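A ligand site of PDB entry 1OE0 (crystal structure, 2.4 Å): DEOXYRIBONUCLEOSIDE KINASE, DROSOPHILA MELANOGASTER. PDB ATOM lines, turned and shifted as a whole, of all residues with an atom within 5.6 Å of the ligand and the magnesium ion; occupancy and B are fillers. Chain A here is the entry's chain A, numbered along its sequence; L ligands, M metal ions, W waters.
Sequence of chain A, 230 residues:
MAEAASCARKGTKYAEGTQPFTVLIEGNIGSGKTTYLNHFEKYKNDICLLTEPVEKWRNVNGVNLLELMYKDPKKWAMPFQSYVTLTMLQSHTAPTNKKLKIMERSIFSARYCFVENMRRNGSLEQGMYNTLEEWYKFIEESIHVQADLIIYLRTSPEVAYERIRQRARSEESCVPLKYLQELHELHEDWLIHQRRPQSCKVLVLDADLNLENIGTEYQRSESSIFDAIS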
ATOM      1  N   GLY A  27      14.286  21.382  15.714  1.00  0.00           N
ATOM      2  CA  GLY A  27      13.067  20.794  15.193  1.00  0.00           C
ATOM      3  C   GLY A  27      12.093  20.633  16.351  1.00  0.00           C
ATOM      4  O   GLY A  27      12.498  20.629  17.515  1.00  0.00           O
ATOM      5  N   ASN A  28      10.819  20.486  16.038  1.00  0.00           N
ATOM      6  CA  ASN A  28       9.801  20.341  17.068  1.00  0.00           C
ATOM      7  C   ASN A  28      10.031  19.106  17.915  1.00  0.00           C
ATOM      8  O   ASN A  28      10.855  18.253  17.563  1.00  0.00           O
ATOM      9  CB  ASN A  28       8.423  20.237  16.414  1.00  0.00           C
ATOM     10  CG  ASN A  28       7.303  20.664  17.341  1.00  0.00           C
ATOM     11  OD1 ASN A  28       7.450  20.682  18.561  1.00  0.00           O
ATOM     12  ND2 ASN A  28       6.156  20.998  16.751  1.00  0.00           N
ATOM     13  N   ILE A  29       9.312  18.996  19.023  1.00  0.00           N
ATOM     14  CA  ILE A  29       9.430  17.823  19.876  1.00  0.00           C
ATOM     15  C   ILE A  29       9.068  16.623  19.008  1.00  0.00           C
ATOM     16  O   ILE A  29       8.067  16.639  18.290  1.00  0.00           O
ATOM     17  CB  ILE A  29       8.433  17.873  21.048  1.00  0.00           C
ATOM     18  CG1 ILE A  29       8.626  19.160  21.851  1.00  0.00           C
ATOM     19  CG2 ILE A  29       8.623  16.655  21.943  1.00  0.00           C
ATOM     20  CD1 ILE A  29       7.587  19.344  22.945  1.00  0.00           C
ATOM     21  N   GLY A  30       9.872  15.571  19.086  1.00  0.00           N
ATOM     22  CA  GLY A  30       9.581  14.375  18.315  1.00  0.00           C
ATOM     23  C   GLY A  30       9.825  14.495  16.828  1.00  0.00           C
ATOM     24  O   GLY A  30       9.356  13.658  16.075  1.00  0.00           O
ATOM     25  N   SER A  31      10.523  15.534  16.384  1.00  0.00           N
ATOM     26  CA  SER A  31      10.804  15.702  14.966  1.00  0.00           C
ATOM     27  C   SER A  31      11.915  14.753  14.499  1.00  0.00           C
ATOM     28  O   SER A  31      12.144  14.587  13.301  1.00  0.00           O
ATOM     29  CB  SER A  31      11.202  17.146  14.674  1.00  0.00           C
ATOM     30  OG  SER A  31      12.358  17.522  15.407  1.00  0.00           O
ATOM     31  N   GLY A  32      12.598  14.120  15.458  1.00  0.00           N
ATOM     32  CA  GLY A  32      13.672  13.196  15.105  1.00  0.00           C
ATOM     33  C   GLY A  32      15.075  13.769  15.171  1.00  0.00           C
ATOM     34  O   GLY A  32      15.958  13.334  14.419  1.00  0.00           O
ATOM     35  N   LYS A  33      15.315  14.725  16.059  1.00  0.00           N
ATOM     36  CA  LYS A  33      16.637  15.329  16.189  1.00  0.00           C
ATOM     37  C   LYS A  33      17.672  14.317  16.645  1.00  0.00           C
ATOM     38  O   LYS A  33      18.795  14.298  16.133  1.00  0.00           O
ATOM     39  CB  LYS A  33      16.603  16.519  17.167  1.00  0.00           C
ATOM     40  CG  LYS A  33      15.739  17.685  16.706  1.00  0.00           C
ATOM     41  CD  LYS A  33      15.721  18.827  17.721  1.00  0.00           C
ATOM     42  CE  LYS A  33      15.040  18.436  19.030  1.00  0.00           C
ATOM     43  NZ  LYS A  33      13.585  18.120  18.852  1.00  0.00           N
ATOM     44  N   THR A  34      17.315  13.481  17.617  1.00  0.00           N
ATOM     45  CA  THR A  34      18.248  12.471  18.122  1.00  0.00           C
ATOM     46  C   THR A  34      18.495  11.392  17.082  1.00  0.00           C
ATOM     47  O   THR A  34      19.635  10.990  16.848  1.00  0.00           O
ATOM     48  CB  THR A  34      17.696  11.831  19.412  1.00  0.00           C
ATOM     49  OG1 THR A  34      17.512  12.843  20.403  1.00  0.00           O
ATOM     50  CG2 THR A  34      18.675  10.772  19.946  1.00  0.00           C
ATOM     51  N   THR A  35      17.415  10.935  16.436  1.00  0.00           N
ATOM     52  CA  THR A  35      17.515   9.909  15.392  1.00  0.00           C
ATOM     53  C   THR A  35      18.483  10.365  14.313  1.00  0.00           C
ATOM     54  O   THR A  35      19.320   9.596  13.850  1.00  0.00           O
ATOM     55  CB  THR A  35      16.145   9.661  14.724  1.00  0.00           C
ATOM     56  OG1 THR A  35      15.225   9.123  15.684  1.00  0.00           O
ATOM     57  CG2 THR A  35      16.289   8.704  13.557  1.00  0.00           C
ATOM     58  N   GLU A  52      20.606  14.275  23.059  1.00  0.00           N
ATOM     59  CA  GLU A  52      19.593  13.980  24.068  1.00  0.00           C
ATOM     60  C   GLU A  52      19.782  14.680  25.415  1.00  0.00           C
ATOM     61  O   GLU A  52      19.915  14.024  26.449  1.00  0.00           O
ATOM     62  CB  GLU A  52      19.533  12.465  24.276  1.00  0.00           C
ATOM     63  CG  GLU A  52      18.198  11.947  24.824  1.00  0.00           C
ATOM     64  CD  GLU A  52      17.057  12.049  23.809  1.00  0.00           C
ATOM     65  OE1 GLU A  52      16.347  11.037  23.612  1.00  0.00           O
ATOM     66  OE2 GLU A  52      16.867  13.154  23.230  1.00  0.00           O
ATOM     67  N   VAL A  54      17.683  16.053  27.214  1.00  0.00           N
ATOM     68  CA  VAL A  54      16.529  15.771  28.075  1.00  0.00           C
ATOM     69  C   VAL A  54      16.875  14.881  29.248  1.00  0.00           C
ATOM     70  O   VAL A  54      16.273  15.006  30.320  1.00  0.00           O
ATOM     71  CB  VAL A  54      15.410  15.069  27.296  1.00  0.00           C
ATOM     72  CG1 VAL A  54      14.075  15.366  27.940  1.00  0.00           C
ATOM     73  CG2 VAL A  54      15.458  15.497  25.836  1.00  0.00           C
ATOM     74  N   TRP A  57      17.648  16.821  32.258  1.00  0.00           N
ATOM     75  CA  TRP A  57      16.484  17.494  32.840  1.00  0.00           C
ATOM     76  C   TRP A  57      15.561  16.525  33.589  1.00  0.00           C
ATOM     77  O   TRP A  57      14.836  16.919  34.489  1.00  0.00           O
ATOM     78  CB  TRP A  57      15.689  18.229  31.746  1.00  0.00           C
ATOM     79  CG  TRP A  57      16.564  19.012  30.821  1.00  0.00           C
ATOM     80  CD1 TRP A  57      17.791  19.545  31.112  1.00  0.00           C
ATOM     81  CD2 TRP A  57      16.300  19.325  29.452  1.00  0.00           C
ATOM     82  NE1 TRP A  57      18.311  20.159  30.001  1.00  0.00           N
ATOM     83  CE2 TRP A  57      17.425  20.045  28.973  1.00  0.00           C
ATOM     84  CE3 TRP A  57      15.237  19.083  28.592  1.00  0.00           C
ATOM     85  CZ2 TRP A  57      17.512  20.510  27.659  1.00  0.00           C
ATOM     86  CZ3 TRP A  57      15.327  19.540  27.283  1.00  0.00           C
ATOM     87  CH2 TRP A  57      16.455  20.251  26.832  1.00  0.00           C
ATOM     88  N   LEU A  66      11.701  17.867  34.377  1.00  0.00           N
ATOM     89  CA  LEU A  66      10.814  17.774  33.219  1.00  0.00           C
ATOM     90  C   LEU A  66       9.420  17.387  33.670  1.00  0.00           C
ATOM     91  O   LEU A  66       8.425  17.972  33.250  1.00  0.00           O
ATOM     92  CB  LEU A  66      11.325  16.736  32.227  1.00  0.00           C
ATOM     93  CG  LEU A  66      10.461  16.623  30.979  1.00  0.00           C
ATOM     94  CD1 LEU A  66      10.469  17.946  30.255  1.00  0.00           C
ATOM     95  CD2 LEU A  66      10.995  15.510  30.084  1.00  0.00           C
ATOM     96  N   MET A  69       7.677  20.163  35.734  1.00  0.00           N
ATOM     97  CA  MET A  69       7.236  21.257  34.883  1.00  0.00           C
ATOM     98  C   MET A  69       5.898  20.947  34.231  1.00  0.00           C
ATOM     99  O   MET A  69       5.014  21.791  34.212  1.00  0.00           O
ATOM    100  CB  MET A  69       8.289  21.549  33.806  1.00  0.00           C
ATOM    101  CG  MET A  69       7.903  22.668  32.831  1.00  0.00           C
ATOM    102  SD  MET A  69       6.909  22.079  31.419  1.00  0.00           S
ATOM    103  CE  MET A  69       8.191  21.274  30.420  1.00  0.00           C
ATOM    104  N   TYR A  70       5.742  19.731  33.698  1.00  0.00           N
ATOM    105  CA  TYR A  70       4.487  19.366  33.056  1.00  0.00           C
ATOM    106  C   TYR A  70       3.321  19.239  34.031  1.00  0.00           C
ATOM    107  O   TYR A  70       2.178  19.545  33.682  1.00  0.00           O
ATOM    108  CB  TYR A  70       4.662  18.057  32.275  1.00  0.00           C
ATOM    109  CG  TYR A  70       5.251  18.259  30.898  1.00  0.00           C
ATOM    110  CD1 TYR A  70       6.405  17.574  30.504  1.00  0.00           C
ATOM    111  CD2 TYR A  70       4.672  19.153  29.998  1.00  0.00           C
ATOM    112  CE1 TYR A  70       6.950  17.772  29.236  1.00  0.00           C
ATOM    113  CE2 TYR A  70       5.217  19.350  28.730  1.00  0.00           C
ATOM    114  CZ  TYR A  70       6.350  18.656  28.359  1.00  0.00           C
ATOM    115  OH  TYR A  70       6.880  18.841  27.102  1.00  0.00           O
ATOM    116  N   PHE A  80      12.702  25.112  35.656  1.00  0.00           N
ATOM    117  CA  PHE A  80      12.995  24.172  34.594  1.00  0.00           C
ATOM    118  C   PHE A  80      13.715  24.840  33.410  1.00  0.00           C
ATOM    119  O   PHE A  80      14.761  24.365  32.982  1.00  0.00           O
ATOM    120  CB  PHE A  80      11.713  23.518  34.068  1.00  0.00           C
ATOM    121  CG  PHE A  80      11.938  22.626  32.865  1.00  0.00           C
ATOM    122  CD1 PHE A  80      12.617  21.421  32.983  1.00  0.00           C
ATOM    123  CD2 PHE A  80      11.501  23.025  31.611  1.00  0.00           C
ATOM    124  CE1 PHE A  80      12.847  20.624  31.878  1.00  0.00           C
ATOM    125  CE2 PHE A  80      11.732  22.229  30.481  1.00  0.00           C
ATOM    126  CZ  PHE A  80      12.410  21.023  30.623  1.00  0.00           C
ATOM    127  N   GLN A  81      13.144  25.942  32.897  1.00  0.00           N
ATOM    128  CA  GLN A  81      13.756  26.647  31.768  1.00  0.00           C
ATOM    129  C   GLN A  81      15.109  27.229  32.151  1.00  0.00           C
ATOM    130  O   GLN A  81      16.013  27.296  31.339  1.00  0.00           O
ATOM    131  CB  GLN A  81      12.813  27.747  31.236  1.00  0.00           C
ATOM    132  CG  GLN A  81      11.611  27.181  30.495  1.00  0.00           C
ATOM    133  CD  GLN A  81      12.007  26.333  29.305  1.00  0.00           C
ATOM    134  OE1 GLN A  81      11.308  25.382  28.951  1.00  0.00           O
ATOM    135  NE2 GLN A  81      13.137  26.672  28.666  1.00  0.00           N
ATOM    136  N   VAL A  84      17.376  24.331  31.775  1.00  0.00           N
ATOM    137  CA  VAL A  84      17.568  24.001  30.362  1.00  0.00           C
ATOM    138  C   VAL A  84      18.619  24.982  29.798  1.00  0.00           C
ATOM    139  O   VAL A  84      19.553  24.589  29.115  1.00  0.00           O
ATOM    140  CB  VAL A  84      16.263  24.180  29.535  1.00  0.00           C
ATOM    141  CG1 VAL A  84      16.596  24.210  28.053  1.00  0.00           C
ATOM    142  CG2 VAL A  84      15.292  23.045  29.823  1.00  0.00           C
ATOM    143  N   GLU A 104      22.233  18.733  19.752  1.00  0.00           N
ATOM    144  CA  GLU A 104      20.772  18.600  19.695  1.00  0.00           C
ATOM    145  C   GLU A 104      20.200  19.762  20.500  1.00  0.00           C
ATOM    146  O   GLU A 104      20.469  19.881  21.700  1.00  0.00           O
ATOM    147  CB  GLU A 104      20.299  17.256  20.269  1.00  0.00           C
ATOM    148  CG  GLU A 104      18.825  16.964  20.058  1.00  0.00           C
ATOM    149  CD  GLU A 104      18.386  15.641  20.646  1.00  0.00           C
ATOM    150  OE1 GLU A 104      19.223  14.721  20.722  1.00  0.00           O
ATOM    151  OE2 GLU A 104      17.202  15.515  21.033  1.00  0.00           O
ATOM    152  N   ARG A 105      19.412  20.611  19.847  1.00  0.00           N
ATOM    153  CA  ARG A 105      18.858  21.770  20.531  1.00  0.00           C
ATOM    154  C   ARG A 105      19.945  22.799  20.796  1.00  0.00           C
ATOM    155  O   ARG A 105      21.116  22.584  20.504  1.00  0.00           O
ATOM    156  CB  ARG A 105      18.218  21.384  21.862  1.00  0.00           C
ATOM    157  CG  ARG A 105      16.845  20.773  21.738  1.00  0.00           C
ATOM    158  CD  ARG A 105      15.886  21.739  21.087  1.00  0.00           C
ATOM    159  NE  ARG A 105      14.535  21.208  21.065  1.00  0.00           N
ATOM    160  CZ  ARG A 105      13.578  21.678  20.262  1.00  0.00           C
ATOM    161  NH1 ARG A 105      13.856  22.680  19.440  1.00  0.00           N
ATOM    162  NH2 ARG A 105      12.356  21.139  20.282  1.00  0.00           N
ATOM    163  N   SER A 106      19.546  23.932  21.382  1.00  0.00           N
ATOM    164  CA  SER A 106      20.458  25.006  21.679  1.00  0.00           C
ATOM    165  C   SER A 106      19.785  25.985  22.618  1.00  0.00           C
ATOM    166  O   SER A 106      18.600  25.885  22.907  1.00  0.00           O
ATOM    167  CB  SER A 106      20.847  25.733  20.394  1.00  0.00           C
ATOM    168  OG  SER A 106      19.715  26.386  19.840  1.00  0.00           O
ATOM    169  N   SER A 109      16.628  27.850  20.863  1.00  0.00           N
ATOM    170  CA  SER A 109      15.303  27.273  20.743  1.00  0.00           C
ATOM    171  C   SER A 109      14.631  27.301  22.103  1.00  0.00           C
ATOM    172  O   SER A 109      13.415  27.367  22.196  1.00  0.00           O
ATOM    173  CB  SER A 109      15.380  25.839  20.191  1.00  0.00           C
ATOM    174  OG  SER A 109      16.350  25.073  20.878  1.00  0.00           O
ATOM    175  N   ALA A 110      15.443  27.250  23.151  1.00  0.00           N
ATOM    176  CA  ALA A 110      14.884  27.300  24.504  1.00  0.00           C
ATOM    177  C   ALA A 110      14.273  28.674  24.710  1.00  0.00           C
ATOM    178  O   ALA A 110      13.174  28.807  25.268  1.00  0.00           O
ATOM    179  CB  ALA A 110      15.980  27.058  25.541  1.00  0.00           C
ATOM    180  N   ARG A 111      14.970  29.709  24.233  1.00  0.00           N
ATOM    181  CA  ARG A 111      14.510  31.082  24.375  1.00  0.00           C
ATOM    182  C   ARG A 111      13.380  31.465  23.420  1.00  0.00           C
ATOM    183  O   ARG A 111      12.291  31.851  23.852  1.00  0.00           O
ATOM    184  CB  ARG A 111      15.668  32.056  24.155  1.00  0.00           C
ATOM    185  CG  ARG A 111      15.277  33.519  24.274  1.00  0.00           C
ATOM    186  CD  ARG A 111      16.416  34.464  23.934  1.00  0.00           C
ATOM    187  NE  ARG A 111      16.107  35.824  24.388  1.00  0.00           N
ATOM    188  CZ  ARG A 111      16.916  36.876  24.251  1.00  0.00           C
ATOM    189  NH1 ARG A 111      18.088  36.747  23.659  1.00  0.00           N
ATOM    190  NH2 ARG A 111      16.559  38.058  24.726  1.00  0.00           N
ATOM    191  N   PHE A 114      10.393  27.724  23.324  1.00  0.00           N
ATOM    192  CA  PHE A 114       9.795  27.289  24.565  1.00  0.00           C
ATOM    193  C   PHE A 114       9.489  28.360  25.591  1.00  0.00           C
ATOM    194  O   PHE A 114       8.379  28.390  26.116  1.00  0.00           O
ATOM    195  CB  PHE A 114      10.644  26.180  25.187  1.00  0.00           C
ATOM    196  CG  PHE A 114      10.676  24.931  24.361  1.00  0.00           C
ATOM    197  CD1 PHE A 114      11.601  24.792  23.343  1.00  0.00           C
ATOM    198  CD2 PHE A 114       9.718  23.944  24.548  1.00  0.00           C
ATOM    199  CE1 PHE A 114      11.561  23.684  22.503  1.00  0.00           C
ATOM    200  CE2 PHE A 114       9.668  22.833  23.712  1.00  0.00           C
ATOM    201  CZ  PHE A 114      10.592  22.708  22.698  1.00  0.00           C
ATOM    202  N   VAL A 115      10.455  29.226  25.899  1.00  0.00           N
ATOM    203  CA  VAL A 115      10.187  30.275  26.868  1.00  0.00           C
ATOM    204  C   VAL A 115       9.090  31.192  26.340  1.00  0.00           C
ATOM    205  O   VAL A 115       8.169  31.564  27.069  1.00  0.00           O
ATOM    206  CB  VAL A 115      11.458  31.119  27.179  1.00  0.00           C
ATOM    207  CG1 VAL A 115      11.076  32.361  27.982  1.00  0.00           C
ATOM    208  CG2 VAL A 115      12.452  30.278  27.963  1.00  0.00           C
ATOM    209  N   MET A 118       5.695  29.574  26.602  1.00  0.00           N
ATOM    210  CA  MET A 118       5.272  29.502  28.001  1.00  0.00           C
ATOM    211  C   MET A 118       4.846  30.865  28.521  1.00  0.00           C
ATOM    212  O   MET A 118       4.073  30.957  29.479  1.00  0.00           O
ATOM    213  CB  MET A 118       6.399  28.932  28.865  1.00  0.00           C
ATOM    214  CG  MET A 118       6.630  27.458  28.616  1.00  0.00           C
ATOM    215  SD  MET A 118       7.985  26.796  29.579  1.00  0.00           S
ATOM    216  CE  MET A 118       8.056  25.093  28.936  1.00  0.00           C
ATOM    217  N   LEU A 153      14.897  20.242  11.220  1.00  0.00           N
ATOM    218  CA  LEU A 153      14.128  19.069  10.835  1.00  0.00           C
ATOM    219  C   LEU A 153      12.658  19.465  10.852  1.00  0.00           C
ATOM    220  O   LEU A 153      11.962  19.317  11.858  1.00  0.00           O
ATOM    221  CB  LEU A 153      14.375  17.909  11.824  1.00  0.00           C
ATOM    222  CG  LEU A 153      15.823  17.447  12.017  1.00  0.00           C
ATOM    223  CD1 LEU A 153      15.828  16.224  12.916  1.00  0.00           C
ATOM    224  CD2 LEU A 153      16.459  17.108  10.682  1.00  0.00           C
ATOM    225  N   ARG A 167       7.213   6.964  21.505  1.00  0.00           N
ATOM    226  CA  ARG A 167       8.358   6.976  22.405  1.00  0.00           C
ATOM    227  C   ARG A 167       7.843   6.735  23.832  1.00  0.00           C
ATOM    228  O   ARG A 167       8.485   6.060  24.636  1.00  0.00           O
ATOM    229  CB  ARG A 167       9.083   8.324  22.320  1.00  0.00           C
ATOM    230  CG  ARG A 167      10.285   8.500  23.240  1.00  0.00           C
ATOM    231  CD  ARG A 167      11.060   9.758  22.813  1.00  0.00           C
ATOM    232  NE  ARG A 167      10.232  10.957  22.870  1.00  0.00           N
ATOM    233  CZ  ARG A 167      10.438  12.041  22.138  1.00  0.00           C
ATOM    234  NH1 ARG A 167      11.446  12.092  21.272  1.00  0.00           N
ATOM    235  NH2 ARG A 167       9.643  13.104  22.277  1.00  0.00           N
ATOM    236  N   ARG A 169       7.362   8.777  26.641  1.00  0.00           N
ATOM    237  CA  ARG A 169       8.033   9.265  27.853  1.00  0.00           C
ATOM    238  C   ARG A 169       6.881   9.578  28.795  1.00  0.00           C
ATOM    239  O   ARG A 169       5.947  10.290  28.439  1.00  0.00           O
ATOM    240  CB  ARG A 169       8.823  10.545  27.588  1.00  0.00           C
ATOM    241  CG  ARG A 169      10.111  10.383  26.795  1.00  0.00           C
ATOM    242  CD  ARG A 169      10.789  11.746  26.630  1.00  0.00           C
ATOM    243  NE  ARG A 169      12.016  11.685  25.830  1.00  0.00           N
ATOM    244  CZ  ARG A 169      12.393  12.646  24.982  1.00  0.00           C
ATOM    245  NH1 ARG A 169      11.652  13.742  24.838  1.00  0.00           N
ATOM    246  NH2 ARG A 169      13.503  12.497  24.277  1.00  0.00           N
ATOM    247  N   GLU A 172       5.731  13.185  29.104  1.00  0.00           N
ATOM    248  CA  GLU A 172       5.049  13.745  27.939  1.00  0.00           C
ATOM    249  C   GLU A 172       3.670  13.146  27.644  1.00  0.00           C
ATOM    250  O   GLU A 172       3.035  13.506  26.641  1.00  0.00           O
ATOM    251  CB  GLU A 172       5.961  13.585  26.710  1.00  0.00           C
ATOM    252  CG  GLU A 172       7.076  14.624  26.642  1.00  0.00           C
ATOM    253  CD  GLU A 172       8.269  14.189  25.808  1.00  0.00           C
ATOM    254  OE1 GLU A 172       8.078  13.486  24.783  1.00  0.00           O
ATOM    255  OE2 GLU A 172       9.402  14.550  26.175  1.00  0.00           O
ATOM    256  N   VAL A 175       0.908  15.818  26.799  1.00  0.00           N
ATOM    257  CA  VAL A 175       1.165  16.865  25.814  1.00  0.00           C
ATOM    258  C   VAL A 175       0.134  16.866  24.686  1.00  0.00           C
ATOM    259  O   VAL A 175       0.064  15.938  23.879  1.00  0.00           O
ATOM    260  CB  VAL A 175       2.587  16.711  25.194  1.00  0.00           C
ATOM    261  CG1 VAL A 175       2.847  17.846  24.216  1.00  0.00           C
ATOM    262  CG2 VAL A 175       3.625  16.708  26.286  1.00  0.00           C
ATOM    263  N   TYR A 179      -0.318  22.189  21.641  1.00  0.00           N
ATOM    264  CA  TYR A 179       0.969  22.583  22.163  1.00  0.00           C
ATOM    265  C   TYR A 179       2.005  22.425  21.079  1.00  0.00           C
ATOM    266  O   TYR A 179       2.803  23.340  20.834  1.00  0.00           O
ATOM    267  CB  TYR A 179       1.335  21.719  23.375  1.00  0.00           C
ATOM    268  CG  TYR A 179       2.549  22.181  24.137  1.00  0.00           C
ATOM    269  CD1 TYR A 179       2.603  23.465  24.706  1.00  0.00           C
ATOM    270  CD2 TYR A 179       3.640  21.335  24.340  1.00  0.00           C
ATOM    271  CE1 TYR A 179       3.698  23.878  25.445  1.00  0.00           C
ATOM    272  CE2 TYR A 179       4.757  21.744  25.076  1.00  0.00           C
ATOM    273  CZ  TYR A 179       4.774  23.015  25.626  1.00  0.00           C
ATOM    274  OH  TYR A 179       5.850  23.437  26.378  1.00  0.00           O
HETATM  275  P1  LIG L   1      13.211  18.222  22.605  1.00  0.00           P
HETATM  276  O1  LIG L   1      14.241  19.192  23.050  1.00  0.00           O
HETATM  277  O2  LIG L   1      12.485  18.499  21.356  1.00  0.00           O
HETATM  278  O3  LIG L   1      13.875  16.785  22.493  1.00  0.00           O
HETATM  279  P2  LIG L   1      13.244  15.408  22.001  1.00  0.00           P
HETATM  280  O4  LIG L   1      14.202  14.379  22.393  1.00  0.00           O
HETATM  281  O5  LIG L   1      11.868  15.284  22.568  1.00  0.00           O
HETATM  282  O6  LIG L   1      13.265  15.552  20.417  1.00  0.00           O
HETATM  283  P3  LIG L   1      13.528  14.557  19.110  1.00  0.00           P
HETATM  284  O7  LIG L   1      12.504  13.494  19.145  1.00  0.00           O
HETATM  285  O8  LIG L   1      13.547  15.399  17.880  1.00  0.00           O
HETATM  286  O9  LIG L   1      14.970  13.941  19.359  1.00  0.00           O
HETATM  287  O10 LIG L   1      12.074  18.048  23.708  1.00  0.00           O
HETATM  288  C1  LIG L   1      12.395  17.303  24.934  1.00  0.00           C
HETATM  289  C2  LIG L   1      11.377  17.642  26.062  1.00  0.00           C
HETATM  290  O11 LIG L   1      11.823  18.826  26.692  1.00  0.00           O
HETATM  291  C3  LIG L   1       9.971  17.951  25.555  1.00  0.00           C
HETATM  292  O12 LIG L   1       9.008  17.386  26.447  1.00  0.00           O
HETATM  293  C4  LIG L   1       9.924  19.493  25.478  1.00  0.00           C
HETATM  294  C5  LIG L   1      10.885  19.862  26.599  1.00  0.00           C
HETATM  295  N1  LIG L   1      11.717  21.132  26.376  1.00  0.00           N
HETATM  296  C6  LIG L   1      11.209  22.245  27.146  1.00  0.00           C
HETATM  297  O13 LIG L   1      10.212  22.149  27.905  1.00  0.00           O
HETATM  298  N2  LIG L   1      11.902  23.435  27.054  1.00  0.00           N
HETATM  299  C7  LIG L   1      12.971  23.581  26.258  1.00  0.00           C
HETATM  300  O14 LIG L   1      13.543  24.800  26.265  1.00  0.00           O
HETATM  301  C8  LIG L   1      13.490  22.471  25.461  1.00  0.00           C
HETATM  302  C9  LIG L   1      14.689  22.636  24.561  1.00  0.00           C
HETATM  303  C10 LIG L   1      12.806  21.302  25.562  1.00  0.00           C
HETATM  304 MG    MG M   1      15.931  13.803  21.273  1.00  0.00          MG
HETATM  305  O   HOH W   1      15.006  11.885  21.209  1.00  0.00           O
HETATM  306  O   HOH W   2      14.662  11.645  17.263  1.00  0.00           O
HETATM  307  O   HOH W   3      11.531  11.833  17.093  1.00  0.00           O
HETATM  308  O   HOH W   4       7.617  21.499  26.894  1.00  0.00           O
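The magnesium ion is bound by OG1 of Thr 34 (2.0 Å), water W1 (2.1 Å), O4 of the ligand (2.1 Å), OE2 of Glu 104 (2.1 Å), O9 of the ligand (2.1 Å) and OE2 of Glu 52 (2.3 Å).
Water W1 bridges the side-chain carboxylate (OE1) of Glu 52 (2.9 Å) and the guanidinium group (NH2) of Arg 169 (3.5 Å). Water W3 lies within hydrogen-bond range of O7 of the ligand (2.8 Å), N of Gly 32 (3.0 Å) and O of Gly 30 (3.0 Å). Water W4 lies within hydrogen-bond range of the side-chain hydroxyl (OH) of Tyr 179 (2.7 Å), the side-chain hydroxyl (OH) of Tyr 70 (2.8 Å) and an oxygen (O13) of the ligand (2.9 Å).
The side-chain amino group (NZ) of Lys 33 is in hydrogen-bond range of the backbone carbonyl oxygen (O) of Asn 28, at 3.0 Å. The backbone carbonyl oxygen (O) of Gly 27 sits at hydrogen-bond distance from the guanidinium group (NH2) of Arg 105, 2.8 Å away. The side-chain carboxylate (OE1) of Glu 172 lies within salt-bridge range of the guanidinium group (NH2) of Arg 167 (3.0 Å). OE1 of Glu 52 lies within salt-bridge range of NH2 of Arg 169 (3.3 Å). The side-chain hydroxyl (OG) of Ser 31 sits at hydrogen-bond distance from the backbone carbonyl oxygen (O) of Asn 28 (2.7 Å). N of Phe 114 sits at hydrogen-bond distance from O of Ser 109 (3.2 Å). The side-chain amide oxygen (OE1) of Gln 81 sits close to the side-chain sulfur (SD) of Met 118, 3.7 Å away. The backbone carbonyl oxygen (O) of Gly 27 is in hydrogen-bond range of the side-chain amino group (NZ) of Lys 33 (3.0 Å).
An oxygen (O12) of the ligand is in hydrogen-bond range of the side-chain hydroxyl (OH) of Tyr 70. N of Gly 32 sits at hydrogen-bond distance from O8 of the ligand (2.9 Å). The guanidinium group (NE) of Arg 105 lies within salt-bridge range of an oxygen (O1) of the ligand (2.8 Å). An oxygen (O7) of the ligand is in salt-bridge range of the guanidinium group (NH1) of Arg 167 (2.8 Å). A nitrogen (N2) of the ligand lies within hydrogen-bond range of the side-chain amide oxygen (OE1) of Gln 81 (2.8 Å). OE2 of Glu 172 sits at hydrogen-bond distance from O12 of the ligand, 2.9 Å away. N of Thr 34 lies close to O9 of the ligand, 3.0 Å away. The side-chain hydroxyl (OG) of Ser 31 is in hydrogen-bond range of an oxygen (O8) of the ligand (3.5 Å). The guanidinium group (NH1) of Arg 169 lies within salt-bridge range of an oxygen (O5) of the ligand (2.8 Å). NZ of Lys 33 is in salt-bridge range of O2 of the ligand, at 2.8 Å. N of Ser 31 is in hydrogen-bond range of O8 of the ligand. An oxygen (O8) of the ligand sits at hydrogen-bond distance from the backbone NH (N) of Lys 33 (2.6 Å). N of Gly 30 lies close to O7 of the ligand, 3.4 Å away.
Within 4 Å of the magnesium ion: Thr 34, Glu 52 and Glu 104.
O of Asn 28 touches O8 of the ligand, 3.9 Å away. CD1 of Ile 29 touches C4 of the ligand (3.4 Å). Val 54 touches the ligand (CG2 to C1, 3.7 Å). Trp 57 touches the ligand. Leu 66 touches the ligand. Met 69 touches the ligand (CE to O13, 3.3 Å). CE2 of Phe 80 touches O13 of the ligand, 3.0 Å away. Val 84 touches the ligand. Ala 110 touches the ligand (CA to O14, 3.3 Å). Phe 114 touches the ligand. Met 118 touches the ligand (CE to O13, 3.8 Å). Hydrophobic or aromatic side chains within 4 Å of the ligand: Ile 29, Val 54, Trp 57, Leu 66, Met 69, Tyr 70, Phe 80, Val 84, Ala 110, Phe 114 and Met 118. Within 4 Å of the ligand: Asn 28, Ile 29, Gly 30, Ser 31, Gly 32, Lys 33, Thr 34, Glu 52, Val 54, Trp 57, Leu 66, Met 69, Tyr 70, Phe 80, Gln 81, Val 84, Glu 104, Arg 105, Ala 110, Phe 114, Met 118, Arg 167, Arg 169 and Glu 172.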
